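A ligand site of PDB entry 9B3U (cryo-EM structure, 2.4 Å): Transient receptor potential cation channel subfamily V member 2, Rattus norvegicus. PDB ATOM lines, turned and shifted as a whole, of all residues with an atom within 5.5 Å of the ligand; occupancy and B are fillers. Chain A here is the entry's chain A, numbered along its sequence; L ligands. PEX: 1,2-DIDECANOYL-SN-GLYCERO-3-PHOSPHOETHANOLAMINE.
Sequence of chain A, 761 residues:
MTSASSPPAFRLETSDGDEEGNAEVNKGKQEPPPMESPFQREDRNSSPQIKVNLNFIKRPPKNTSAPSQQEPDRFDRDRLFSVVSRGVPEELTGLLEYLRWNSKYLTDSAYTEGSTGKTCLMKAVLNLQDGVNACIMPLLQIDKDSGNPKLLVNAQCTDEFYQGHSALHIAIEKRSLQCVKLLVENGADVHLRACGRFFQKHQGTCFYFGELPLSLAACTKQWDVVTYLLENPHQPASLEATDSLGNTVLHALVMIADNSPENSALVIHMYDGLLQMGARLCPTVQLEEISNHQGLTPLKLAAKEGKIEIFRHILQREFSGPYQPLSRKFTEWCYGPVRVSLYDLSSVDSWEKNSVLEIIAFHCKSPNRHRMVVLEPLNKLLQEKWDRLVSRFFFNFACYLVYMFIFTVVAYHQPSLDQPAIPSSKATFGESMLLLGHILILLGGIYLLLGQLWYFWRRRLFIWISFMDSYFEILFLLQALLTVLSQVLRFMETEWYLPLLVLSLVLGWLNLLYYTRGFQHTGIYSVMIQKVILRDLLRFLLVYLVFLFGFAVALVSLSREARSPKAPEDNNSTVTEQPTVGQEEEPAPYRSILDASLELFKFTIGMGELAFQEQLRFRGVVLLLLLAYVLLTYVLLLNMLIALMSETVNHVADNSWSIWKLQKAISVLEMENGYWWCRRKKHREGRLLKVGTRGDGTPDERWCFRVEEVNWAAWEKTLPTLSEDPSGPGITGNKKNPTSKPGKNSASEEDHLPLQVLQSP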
ATOM      1  N   PHE A 395       9.085  14.035  -2.201  1.00  0.00           N
ATOM      2  CA  PHE A 395       9.998  13.760  -1.092  1.00  0.00           C
ATOM      3  C   PHE A 395       9.742  12.384  -0.456  1.00  0.00           C
ATOM      4  O   PHE A 395      10.682  11.633  -0.215  1.00  0.00           O
ATOM      5  CB  PHE A 395       9.880  14.877  -0.047  1.00  0.00           C
ATOM      6  CG  PHE A 395      10.685  14.613   1.201  1.00  0.00           C
ATOM      7  CD1 PHE A 395      12.081  14.791   1.180  1.00  0.00           C
ATOM      8  CD2 PHE A 395      10.059  14.160   2.379  1.00  0.00           C
ATOM      9  CE1 PHE A 395      12.844  14.520   2.327  1.00  0.00           C
ATOM     10  CE2 PHE A 395      10.820  13.902   3.524  1.00  0.00           C
ATOM     11  CZ  PHE A 395      12.216  14.080   3.503  1.00  0.00           C
ATOM     12  N   ASN A 396       8.485  12.007  -0.221  1.00  0.00           N
ATOM     13  CA  ASN A 396       8.128  10.675   0.284  1.00  0.00           C
ATOM     14  C   ASN A 396       8.548   9.558  -0.684  1.00  0.00           C
ATOM     15  O   ASN A 396       9.106   8.551  -0.260  1.00  0.00           O
ATOM     16  CB  ASN A 396       6.614  10.618   0.558  1.00  0.00           C
ATOM     17  CG  ASN A 396       6.143  11.473   1.716  1.00  0.00           C
ATOM     18  OD1 ASN A 396       6.901  11.961   2.527  1.00  0.00           O
ATOM     19  ND2 ASN A 396       4.842  11.653   1.847  1.00  0.00           N
ATOM     20  N   PHE A 397       8.339   9.761  -1.992  1.00  0.00           N
ATOM     21  CA  PHE A 397       8.830   8.867  -3.043  1.00  0.00           C
ATOM     22  C   PHE A 397      10.358   8.749  -3.047  1.00  0.00           C
ATOM     23  O   PHE A 397      10.874   7.636  -3.094  1.00  0.00           O
ATOM     24  CB  PHE A 397       8.364   9.390  -4.404  1.00  0.00           C
ATOM     25  CG  PHE A 397       8.973   8.702  -5.604  1.00  0.00           C
ATOM     26  CD1 PHE A 397       8.807   7.323  -5.796  1.00  0.00           C
ATOM     27  CD2 PHE A 397       9.729   9.432  -6.528  1.00  0.00           C
ATOM     28  CE1 PHE A 397       9.322   6.687  -6.935  1.00  0.00           C
ATOM     29  CE2 PHE A 397      10.294   8.800  -7.647  1.00  0.00           C
ATOM     30  CZ  PHE A 397      10.062   7.428  -7.862  1.00  0.00           C
ATOM     31  N   CYS A 399      12.458   9.264  -0.527  1.00  0.00           N
ATOM     32  CA  CYS A 399      12.824   8.506   0.675  1.00  0.00           C
ATOM     33  C   CYS A 399      12.569   7.008   0.510  1.00  0.00           C
ATOM     34  O   CYS A 399      13.391   6.195   0.940  1.00  0.00           O
ATOM     35  CB  CYS A 399      12.098   9.070   1.892  1.00  0.00           C
ATOM     36  SG  CYS A 399      12.651  10.775   2.164  1.00  0.00           S
ATOM     37  N   TYR A 400      11.469   6.606  -0.149  1.00  0.00           N
ATOM     38  CA  TYR A 400      11.207   5.198  -0.429  1.00  0.00           C
ATOM     39  C   TYR A 400      12.148   4.632  -1.500  1.00  0.00           C
ATOM     40  O   TYR A 400      12.623   3.512  -1.354  1.00  0.00           O
ATOM     41  CB  TYR A 400       9.737   4.976  -0.767  1.00  0.00           C
ATOM     42  CG  TYR A 400       9.312   3.520  -0.628  1.00  0.00           C
ATOM     43  CD1 TYR A 400       9.251   2.938   0.651  1.00  0.00           C
ATOM     44  CD2 TYR A 400       9.028   2.739  -1.761  1.00  0.00           C
ATOM     45  CE1 TYR A 400       8.933   1.579   0.797  1.00  0.00           C
ATOM     46  CE2 TYR A 400       8.681   1.376  -1.615  1.00  0.00           C
ATOM     47  CZ  TYR A 400       8.648   0.799  -0.326  1.00  0.00           C
ATOM     48  OH  TYR A 400       8.328  -0.504  -0.147  1.00  0.00           O
ATOM     49  N   LEU A 401      12.503   5.407  -2.529  1.00  0.00           N
ATOM     50  CA  LEU A 401      13.550   5.042  -3.476  1.00  0.00           C
ATOM     51  C   LEU A 401      14.902   4.834  -2.803  1.00  0.00           C
ATOM     52  O   LEU A 401      15.556   3.837  -3.077  1.00  0.00           O
ATOM     53  CB  LEU A 401      13.733   6.138  -4.547  1.00  0.00           C
ATOM     54  CG  LEU A 401      12.928   5.983  -5.833  1.00  0.00           C
ATOM     55  CD1 LEU A 401      13.326   7.128  -6.755  1.00  0.00           C
ATOM     56  CD2 LEU A 401      13.226   4.687  -6.574  1.00  0.00           C
ATOM     57  N   TYR A 403      15.489   4.140   0.456  1.00  0.00           N
ATOM     58  CA  TYR A 403      15.289   2.915   1.222  1.00  0.00           C
ATOM     59  C   TYR A 403      15.359   1.656   0.339  1.00  0.00           C
ATOM     60  O   TYR A 403      16.110   0.744   0.661  1.00  0.00           O
ATOM     61  CB  TYR A 403      13.986   3.038   2.028  1.00  0.00           C
ATOM     62  CG  TYR A 403      13.457   1.759   2.634  1.00  0.00           C
ATOM     63  CD1 TYR A 403      14.010   1.222   3.817  1.00  0.00           C
ATOM     64  CD2 TYR A 403      12.367   1.106   2.024  1.00  0.00           C
ATOM     65  CE1 TYR A 403      13.440   0.072   4.402  1.00  0.00           C
ATOM     66  CE2 TYR A 403      11.803  -0.038   2.598  1.00  0.00           C
ATOM     67  CZ  TYR A 403      12.316  -0.540   3.815  1.00  0.00           C
ATOM     68  OH  TYR A 403      11.691  -1.571   4.433  1.00  0.00           O
ATOM     69  N   LEU A 443      15.560   0.007  10.610  1.00  0.00           N
ATOM     70  CA  LEU A 443      14.949   1.286  10.984  1.00  0.00           C
ATOM     71  C   LEU A 443      13.905   1.759   9.974  1.00  0.00           C
ATOM     72  O   LEU A 443      12.820   2.165  10.379  1.00  0.00           O
ATOM     73  CB  LEU A 443      16.043   2.353  11.169  1.00  0.00           C
ATOM     74  CG  LEU A 443      16.942   2.129  12.392  1.00  0.00           C
ATOM     75  CD1 LEU A 443      18.107   3.110  12.318  1.00  0.00           C
ATOM     76  CD2 LEU A 443      16.205   2.352  13.710  1.00  0.00           C
ATOM     77  N   GLY A 444      14.174   1.646   8.671  1.00  0.00           N
ATOM     78  CA  GLY A 444      13.184   1.911   7.622  1.00  0.00           C
ATOM     79  C   GLY A 444      11.985   0.968   7.690  1.00  0.00           C
ATOM     80  O   GLY A 444      10.849   1.415   7.562  1.00  0.00           O
ATOM     81  N   TYR A 447      10.020   2.149  10.855  1.00  0.00           N
ATOM     82  CA  TYR A 447       9.359   3.404  10.503  1.00  0.00           C
ATOM     83  C   TYR A 447       8.134   3.202   9.621  1.00  0.00           C
ATOM     84  O   TYR A 447       7.066   3.732   9.916  1.00  0.00           O
ATOM     85  CB  TYR A 447      10.375   4.309   9.801  1.00  0.00           C
ATOM     86  CG  TYR A 447       9.801   5.642   9.399  1.00  0.00           C
ATOM     87  CD1 TYR A 447       9.862   6.708  10.303  1.00  0.00           C
ATOM     88  CD2 TYR A 447       9.189   5.813   8.149  1.00  0.00           C
ATOM     89  CE1 TYR A 447       9.330   7.956   9.965  1.00  0.00           C
ATOM     90  CE2 TYR A 447       8.636   7.063   7.800  1.00  0.00           C
ATOM     91  CZ  TYR A 447       8.711   8.132   8.714  1.00  0.00           C
ATOM     92  OH  TYR A 447       8.165   9.333   8.413  1.00  0.00           O
ATOM     93  N   LEU A 448       8.252   2.407   8.558  1.00  0.00           N
ATOM     94  CA  LEU A 448       7.141   2.073   7.688  1.00  0.00           C
ATOM     95  C   LEU A 448       6.068   1.264   8.415  1.00  0.00           C
ATOM     96  O   LEU A 448       4.883   1.515   8.234  1.00  0.00           O
ATOM     97  CB  LEU A 448       7.660   1.322   6.454  1.00  0.00           C
ATOM     98  CG  LEU A 448       8.470   2.207   5.498  1.00  0.00           C
ATOM     99  CD1 LEU A 448       9.262   1.318   4.553  1.00  0.00           C
ATOM    100  CD2 LEU A 448       7.593   3.131   4.666  1.00  0.00           C
ATOM    101  N   GLN A 452       2.284   2.613   9.074  1.00  0.00           N
ATOM    102  CA  GLN A 452       1.147   1.849   8.499  1.00  0.00           C
ATOM    103  C   GLN A 452       0.198   1.403   9.630  1.00  0.00           C
ATOM    104  O   GLN A 452      -1.021   1.554   9.443  1.00  0.00           O
ATOM    105  CB  GLN A 452       1.707   0.747   7.582  1.00  0.00           C
ATOM    106  CG  GLN A 452       2.338   1.349   6.321  1.00  0.00           C
ATOM    107  CD  GLN A 452       1.285   1.793   5.325  1.00  0.00           C
ATOM    108  OE1 GLN A 452       0.108   1.493   5.459  1.00  0.00           O
ATOM    109  NE2 GLN A 452       1.720   2.508   4.296  1.00  0.00           N
ATOM    110  N   PHE A 472      -2.397  -0.870  -1.466  1.00  0.00           N
ATOM    111  CA  PHE A 472      -1.023  -0.494  -1.163  1.00  0.00           C
ATOM    112  C   PHE A 472      -0.807  -0.228   0.319  1.00  0.00           C
ATOM    113  O   PHE A 472       0.294  -0.440   0.795  1.00  0.00           O
ATOM    114  CB  PHE A 472      -0.586   0.722  -1.993  1.00  0.00           C
ATOM    115  CG  PHE A 472      -0.056   0.357  -3.365  1.00  0.00           C
ATOM    116  CD1 PHE A 472       1.120  -0.401  -3.462  1.00  0.00           C
ATOM    117  CD2 PHE A 472      -0.697   0.811  -4.526  1.00  0.00           C
ATOM    118  CE1 PHE A 472       1.632  -0.737  -4.717  1.00  0.00           C
ATOM    119  CE2 PHE A 472      -0.168   0.499  -5.785  1.00  0.00           C
ATOM    120  CZ  PHE A 472       0.991  -0.282  -5.879  1.00  0.00           C
ATOM    121  N   GLU A 473      -1.819   0.138   1.095  1.00  0.00           N
ATOM    122  CA  GLU A 473      -1.677   0.229   2.550  1.00  0.00           C
ATOM    123  C   GLU A 473      -1.500  -1.166   3.186  1.00  0.00           C
ATOM    124  O   GLU A 473      -0.732  -1.345   4.127  1.00  0.00           O
ATOM    125  CB  GLU A 473      -2.859   0.998   3.151  1.00  0.00           C
ATOM    126  CG  GLU A 473      -3.092   2.388   2.535  1.00  0.00           C
ATOM    127  CD  GLU A 473      -1.886   3.334   2.619  1.00  0.00           C
ATOM    128  OE1 GLU A 473      -1.321   3.551   3.709  1.00  0.00           O
ATOM    129  OE2 GLU A 473      -1.473   3.874   1.565  1.00  0.00           O
ATOM    130  N   PHE A 476       2.355  -2.122   1.752  1.00  0.00           N
ATOM    131  CA  PHE A 476       3.379  -1.413   2.515  1.00  0.00           C
ATOM    132  C   PHE A 476       3.482  -1.945   3.951  1.00  0.00           C
ATOM    133  O   PHE A 476       4.591  -2.111   4.442  1.00  0.00           O
ATOM    134  CB  PHE A 476       3.123   0.100   2.497  1.00  0.00           C
ATOM    135  CG  PHE A 476       3.746   0.846   1.335  1.00  0.00           C
ATOM    136  CD1 PHE A 476       3.164   0.828   0.053  1.00  0.00           C
ATOM    137  CD2 PHE A 476       4.919   1.595   1.539  1.00  0.00           C
ATOM    138  CE1 PHE A 476       3.715   1.580  -0.989  1.00  0.00           C
ATOM    139  CE2 PHE A 476       5.479   2.340   0.488  1.00  0.00           C
ATOM    140  CZ  PHE A 476       4.871   2.344  -0.768  1.00  0.00           C
ATOM    141  N   TYR A 514       3.029   2.431  -6.398  1.00  0.00           N
ATOM    142  CA  TYR A 514       2.141   3.379  -5.726  1.00  0.00           C
ATOM    143  C   TYR A 514       2.338   4.817  -6.230  1.00  0.00           C
ATOM    144  O   TYR A 514       1.386   5.499  -6.572  1.00  0.00           O
ATOM    145  CB  TYR A 514       2.375   3.298  -4.213  1.00  0.00           C
ATOM    146  CG  TYR A 514       1.664   4.357  -3.424  1.00  0.00           C
ATOM    147  CD1 TYR A 514       0.306   4.216  -3.104  1.00  0.00           C
ATOM    148  CD2 TYR A 514       2.348   5.537  -3.071  1.00  0.00           C
ATOM    149  CE1 TYR A 514      -0.369   5.267  -2.445  1.00  0.00           C
ATOM    150  CE2 TYR A 514       1.679   6.593  -2.442  1.00  0.00           C
ATOM    151  CZ  TYR A 514       0.314   6.456  -2.134  1.00  0.00           C
ATOM    152  OH  TYR A 514      -0.348   7.467  -1.518  1.00  0.00           O
ATOM    153  N   TYR A 515       3.592   5.267  -6.315  1.00  0.00           N
ATOM    154  CA  TYR A 515       3.935   6.646  -6.635  1.00  0.00           C
ATOM    155  C   TYR A 515       3.704   7.031  -8.103  1.00  0.00           C
ATOM    156  O   TYR A 515       3.794   8.193  -8.456  1.00  0.00           O
ATOM    157  CB  TYR A 515       5.372   6.945  -6.188  1.00  0.00           C
ATOM    158  CG  TYR A 515       5.602   6.699  -4.711  1.00  0.00           C
ATOM    159  CD1 TYR A 515       5.269   7.675  -3.761  1.00  0.00           C
ATOM    160  CD2 TYR A 515       6.138   5.470  -4.305  1.00  0.00           C
ATOM    161  CE1 TYR A 515       5.478   7.432  -2.386  1.00  0.00           C
ATOM    162  CE2 TYR A 515       6.355   5.219  -2.939  1.00  0.00           C
ATOM    163  CZ  TYR A 515       6.028   6.204  -1.980  1.00  0.00           C
ATOM    164  OH  TYR A 515       6.236   5.913  -0.679  1.00  0.00           O
ATOM    165  N   TYR A 675       3.212  13.202   9.281  1.00  0.00           N
ATOM    166  CA  TYR A 675       3.740  11.881   9.619  1.00  0.00           C
ATOM    167  C   TYR A 675       3.319  11.406  11.017  1.00  0.00           C
ATOM    168  O   TYR A 675       2.996  12.225  11.880  1.00  0.00           O
ATOM    169  CB  TYR A 675       5.272  11.919   9.491  1.00  0.00           C
ATOM    170  CG  TYR A 675       5.754  12.420   8.151  1.00  0.00           C
ATOM    171  CD1 TYR A 675       5.493  11.668   6.994  1.00  0.00           C
ATOM    172  CD2 TYR A 675       6.483  13.621   8.066  1.00  0.00           C
ATOM    173  CE1 TYR A 675       5.932  12.125   5.741  1.00  0.00           C
ATOM    174  CE2 TYR A 675       6.936  14.080   6.813  1.00  0.00           C
ATOM    175  CZ  TYR A 675       6.667  13.334   5.655  1.00  0.00           C
ATOM    176  OH  TYR A 675       7.107  13.782   4.443  1.00  0.00           O
ATOM    177  N   TRP A 676       3.386  10.104  11.284  1.00  0.00           N
ATOM    178  CA  TRP A 676       2.985   9.497  12.560  1.00  0.00           C
ATOM    179  C   TRP A 676       3.713  10.098  13.768  1.00  0.00           C
ATOM    180  O   TRP A 676       3.125  10.228  14.840  1.00  0.00           O
ATOM    181  CB  TRP A 676       3.185   7.976  12.487  1.00  0.00           C
ATOM    182  CG  TRP A 676       4.588   7.458  12.358  1.00  0.00           C
ATOM    183  CD1 TRP A 676       5.213   7.177  11.198  1.00  0.00           C
ATOM    184  CD2 TRP A 676       5.571   7.199  13.406  1.00  0.00           C
ATOM    185  NE1 TRP A 676       6.503   6.757  11.447  1.00  0.00           N
ATOM    186  CE2 TRP A 676       6.785   6.781  12.793  1.00  0.00           C
ATOM    187  CE3 TRP A 676       5.564   7.283  14.819  1.00  0.00           C
ATOM    188  CZ2 TRP A 676       7.946   6.510  13.533  1.00  0.00           C
ATOM    189  CZ3 TRP A 676       6.725   7.013  15.569  1.00  0.00           C
ATOM    190  CH2 TRP A 676       7.911   6.637  14.929  1.00  0.00           C
ATOM    191  N   TRP A 677       4.957  10.518  13.587  1.00  0.00           N
ATOM    192  CA  TRP A 677       5.824  11.139  14.593  1.00  0.00           C
ATOM    193  C   TRP A 677       5.759  12.668  14.626  1.00  0.00           C
ATOM    194  O   TRP A 677       6.263  13.273  15.567  1.00  0.00           O
ATOM    195  CB  TRP A 677       7.260  10.684  14.273  1.00  0.00           C
ATOM    196  CG  TRP A 677       7.757  11.085  12.928  1.00  0.00           C
ATOM    197  CD1 TRP A 677       7.607  10.355  11.800  1.00  0.00           C
ATOM    198  CD2 TRP A 677       8.445  12.309  12.515  1.00  0.00           C
ATOM    199  NE1 TRP A 677       8.124  11.055  10.734  1.00  0.00           N
ATOM    200  CE2 TRP A 677       8.623  12.275  11.108  1.00  0.00           C
ATOM    201  CE3 TRP A 677       8.908  13.448  13.203  1.00  0.00           C
ATOM    202  CZ2 TRP A 677       9.215  13.331  10.405  1.00  0.00           C
ATOM    203  CZ3 TRP A 677       9.528  14.509  12.500  1.00  0.00           C
ATOM    204  CH2 TRP A 677       9.674  14.450  11.106  1.00  0.00           C
HETATM  205  O1  PEX L   1       3.971   8.212   1.434  1.00  0.00           O
HETATM  206  O2  PEX L   1       4.828   8.199   3.707  1.00  0.00           O
HETATM  207  P1  PEX L   1       4.785   7.468   2.420  1.00  0.00           P
HETATM  208  O3  PEX L   1       6.263   7.150   1.858  1.00  0.00           O
HETATM  209  C1  PEX L   1       7.224   6.422   2.652  1.00  0.00           C
HETATM  210  C2  PEX L   1       8.430   7.329   3.004  1.00  0.00           C
HETATM  211  C3  PEX L   1       7.982   8.668   3.605  1.00  0.00           C
HETATM  212  O4  PEX L   1       9.171   9.450   3.773  1.00  0.00           O
HETATM  213  C4  PEX L   1       9.361  10.105   4.933  1.00  0.00           C
HETATM  214  O5  PEX L   1       8.600  10.057   5.876  1.00  0.00           O
HETATM  215  C5  PEX L   1      10.716  10.781   4.948  1.00  0.00           C
HETATM  216  C6  PEX L   1      11.093  11.483   6.276  1.00  0.00           C
HETATM  217  C7  PEX L   1      11.721  10.505   7.294  1.00  0.00           C
HETATM  218  C8  PEX L   1      11.861  11.164   8.674  1.00  0.00           C
HETATM  219  C9  PEX L   1      12.397  10.188   9.750  1.00  0.00           C
HETATM  220  C10 PEX L   1      12.062  10.679  11.177  1.00  0.00           C
HETATM  221  C11 PEX L   1      12.181   9.572  12.245  1.00  0.00           C
HETATM  222  C12 PEX L   1      11.372   9.891  13.507  1.00  0.00           C
HETATM  223  C13 PEX L   1      11.361   8.747  14.517  1.00  0.00           C
HETATM  224  O6  PEX L   1       9.256   6.692   4.014  1.00  0.00           O
HETATM  225  C14 PEX L   1      10.270   5.867   3.641  1.00  0.00           C
HETATM  226  O7  PEX L   1      10.509   5.586   2.504  1.00  0.00           O
HETATM  227  C15 PEX L   1      11.171   5.444   4.792  1.00  0.00           C
HETATM  228  C16 PEX L   1      12.463   6.295   4.831  1.00  0.00           C
HETATM  229  C17 PEX L   1      13.624   5.615   5.591  1.00  0.00           C
HETATM  230  C18 PEX L   1      13.507   5.671   7.128  1.00  0.00           C
HETATM  231  C19 PEX L   1      13.789   7.059   7.735  1.00  0.00           C
HETATM  232  C20 PEX L   1      14.485   6.995   9.123  1.00  0.00           C
HETATM  233  C21 PEX L   1      13.644   6.261  10.197  1.00  0.00           C
HETATM  234  C22 PEX L   1      14.278   6.320  11.606  1.00  0.00           C
HETATM  235  C23 PEX L   1      13.406   5.606  12.657  1.00  0.00           C
HETATM  236  O8  PEX L   1       4.268   5.964   2.624  1.00  0.00           O
HETATM  237  C24 PEX L   1       3.622   5.212   1.572  1.00  0.00           C
HETATM  238  C25 PEX L   1       2.089   5.362   1.703  1.00  0.00           C
HETATM  239  N1  PEX L   1       1.386   4.647   0.623  1.00  0.00           N
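OH of Tyr 447 lies within hydrogen-bond range of O5 of the ligand (2.7 Å).
An oxygen (O3) of the ligand sits at hydrogen-bond distance from the side-chain hydroxyl (OH) of Tyr 515, at 2.8 Å.
N of Tyr 400 lies within hydrogen-bond range of O7 of the ligand, 3.0 Å away.
OE2 of Glu 473 is in salt-bridge range of N1 of the ligand (3.1 Å).
The indole nitrogen (NE1) of Trp 677 lies within hydrogen-bond range of the side-chain hydroxyl (OH) of Tyr 447, 2.9 Å away.
O of Tyr 447 sits close to NE1 of Trp 676 (3.4 Å).
The side-chain carboxylate of Glu 473 lies close to the side-chain amide oxygen of Gln 452 (3.1 Å).
SG of Cys 399 sits at hydrogen-bond distance from O of Phe 395.
OD1 of Asn 396 lies within hydrogen-bond range of OH of Tyr 675, at 2.7 Å.
An oxygen (O7) of the ligand sits close to the backbone carbonyl oxygen of Cys 399, 3.3 Å away.
Phe 395 touches the ligand.
Asn 396 touches the ligand.
Gly 444 touches the ligand.
CD2 of Leu 448 touches C1 of the ligand (3.9 Å).
Gln 452 touches the ligand (NE2 to C25, 3.9 Å).
Phe 476 touches the ligand.
Tyr 514 touches the ligand (CZ to N1, 3.5 Å).
Tyr 675 touches the ligand (CE1 to O5, 3.4 Å).
Trp 677 touches the ligand (CE2 to C10, 3.8 Å).
Hydrophobic or aromatic side chains within 4 Å of the ligand: Phe 395, Tyr 400, Tyr 447, Leu 448, Phe 476, Tyr 514, Tyr 515, Tyr 675 and Trp 677.
Along chain A the residues within 4 Å of the ligand span positions 395 to 677.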
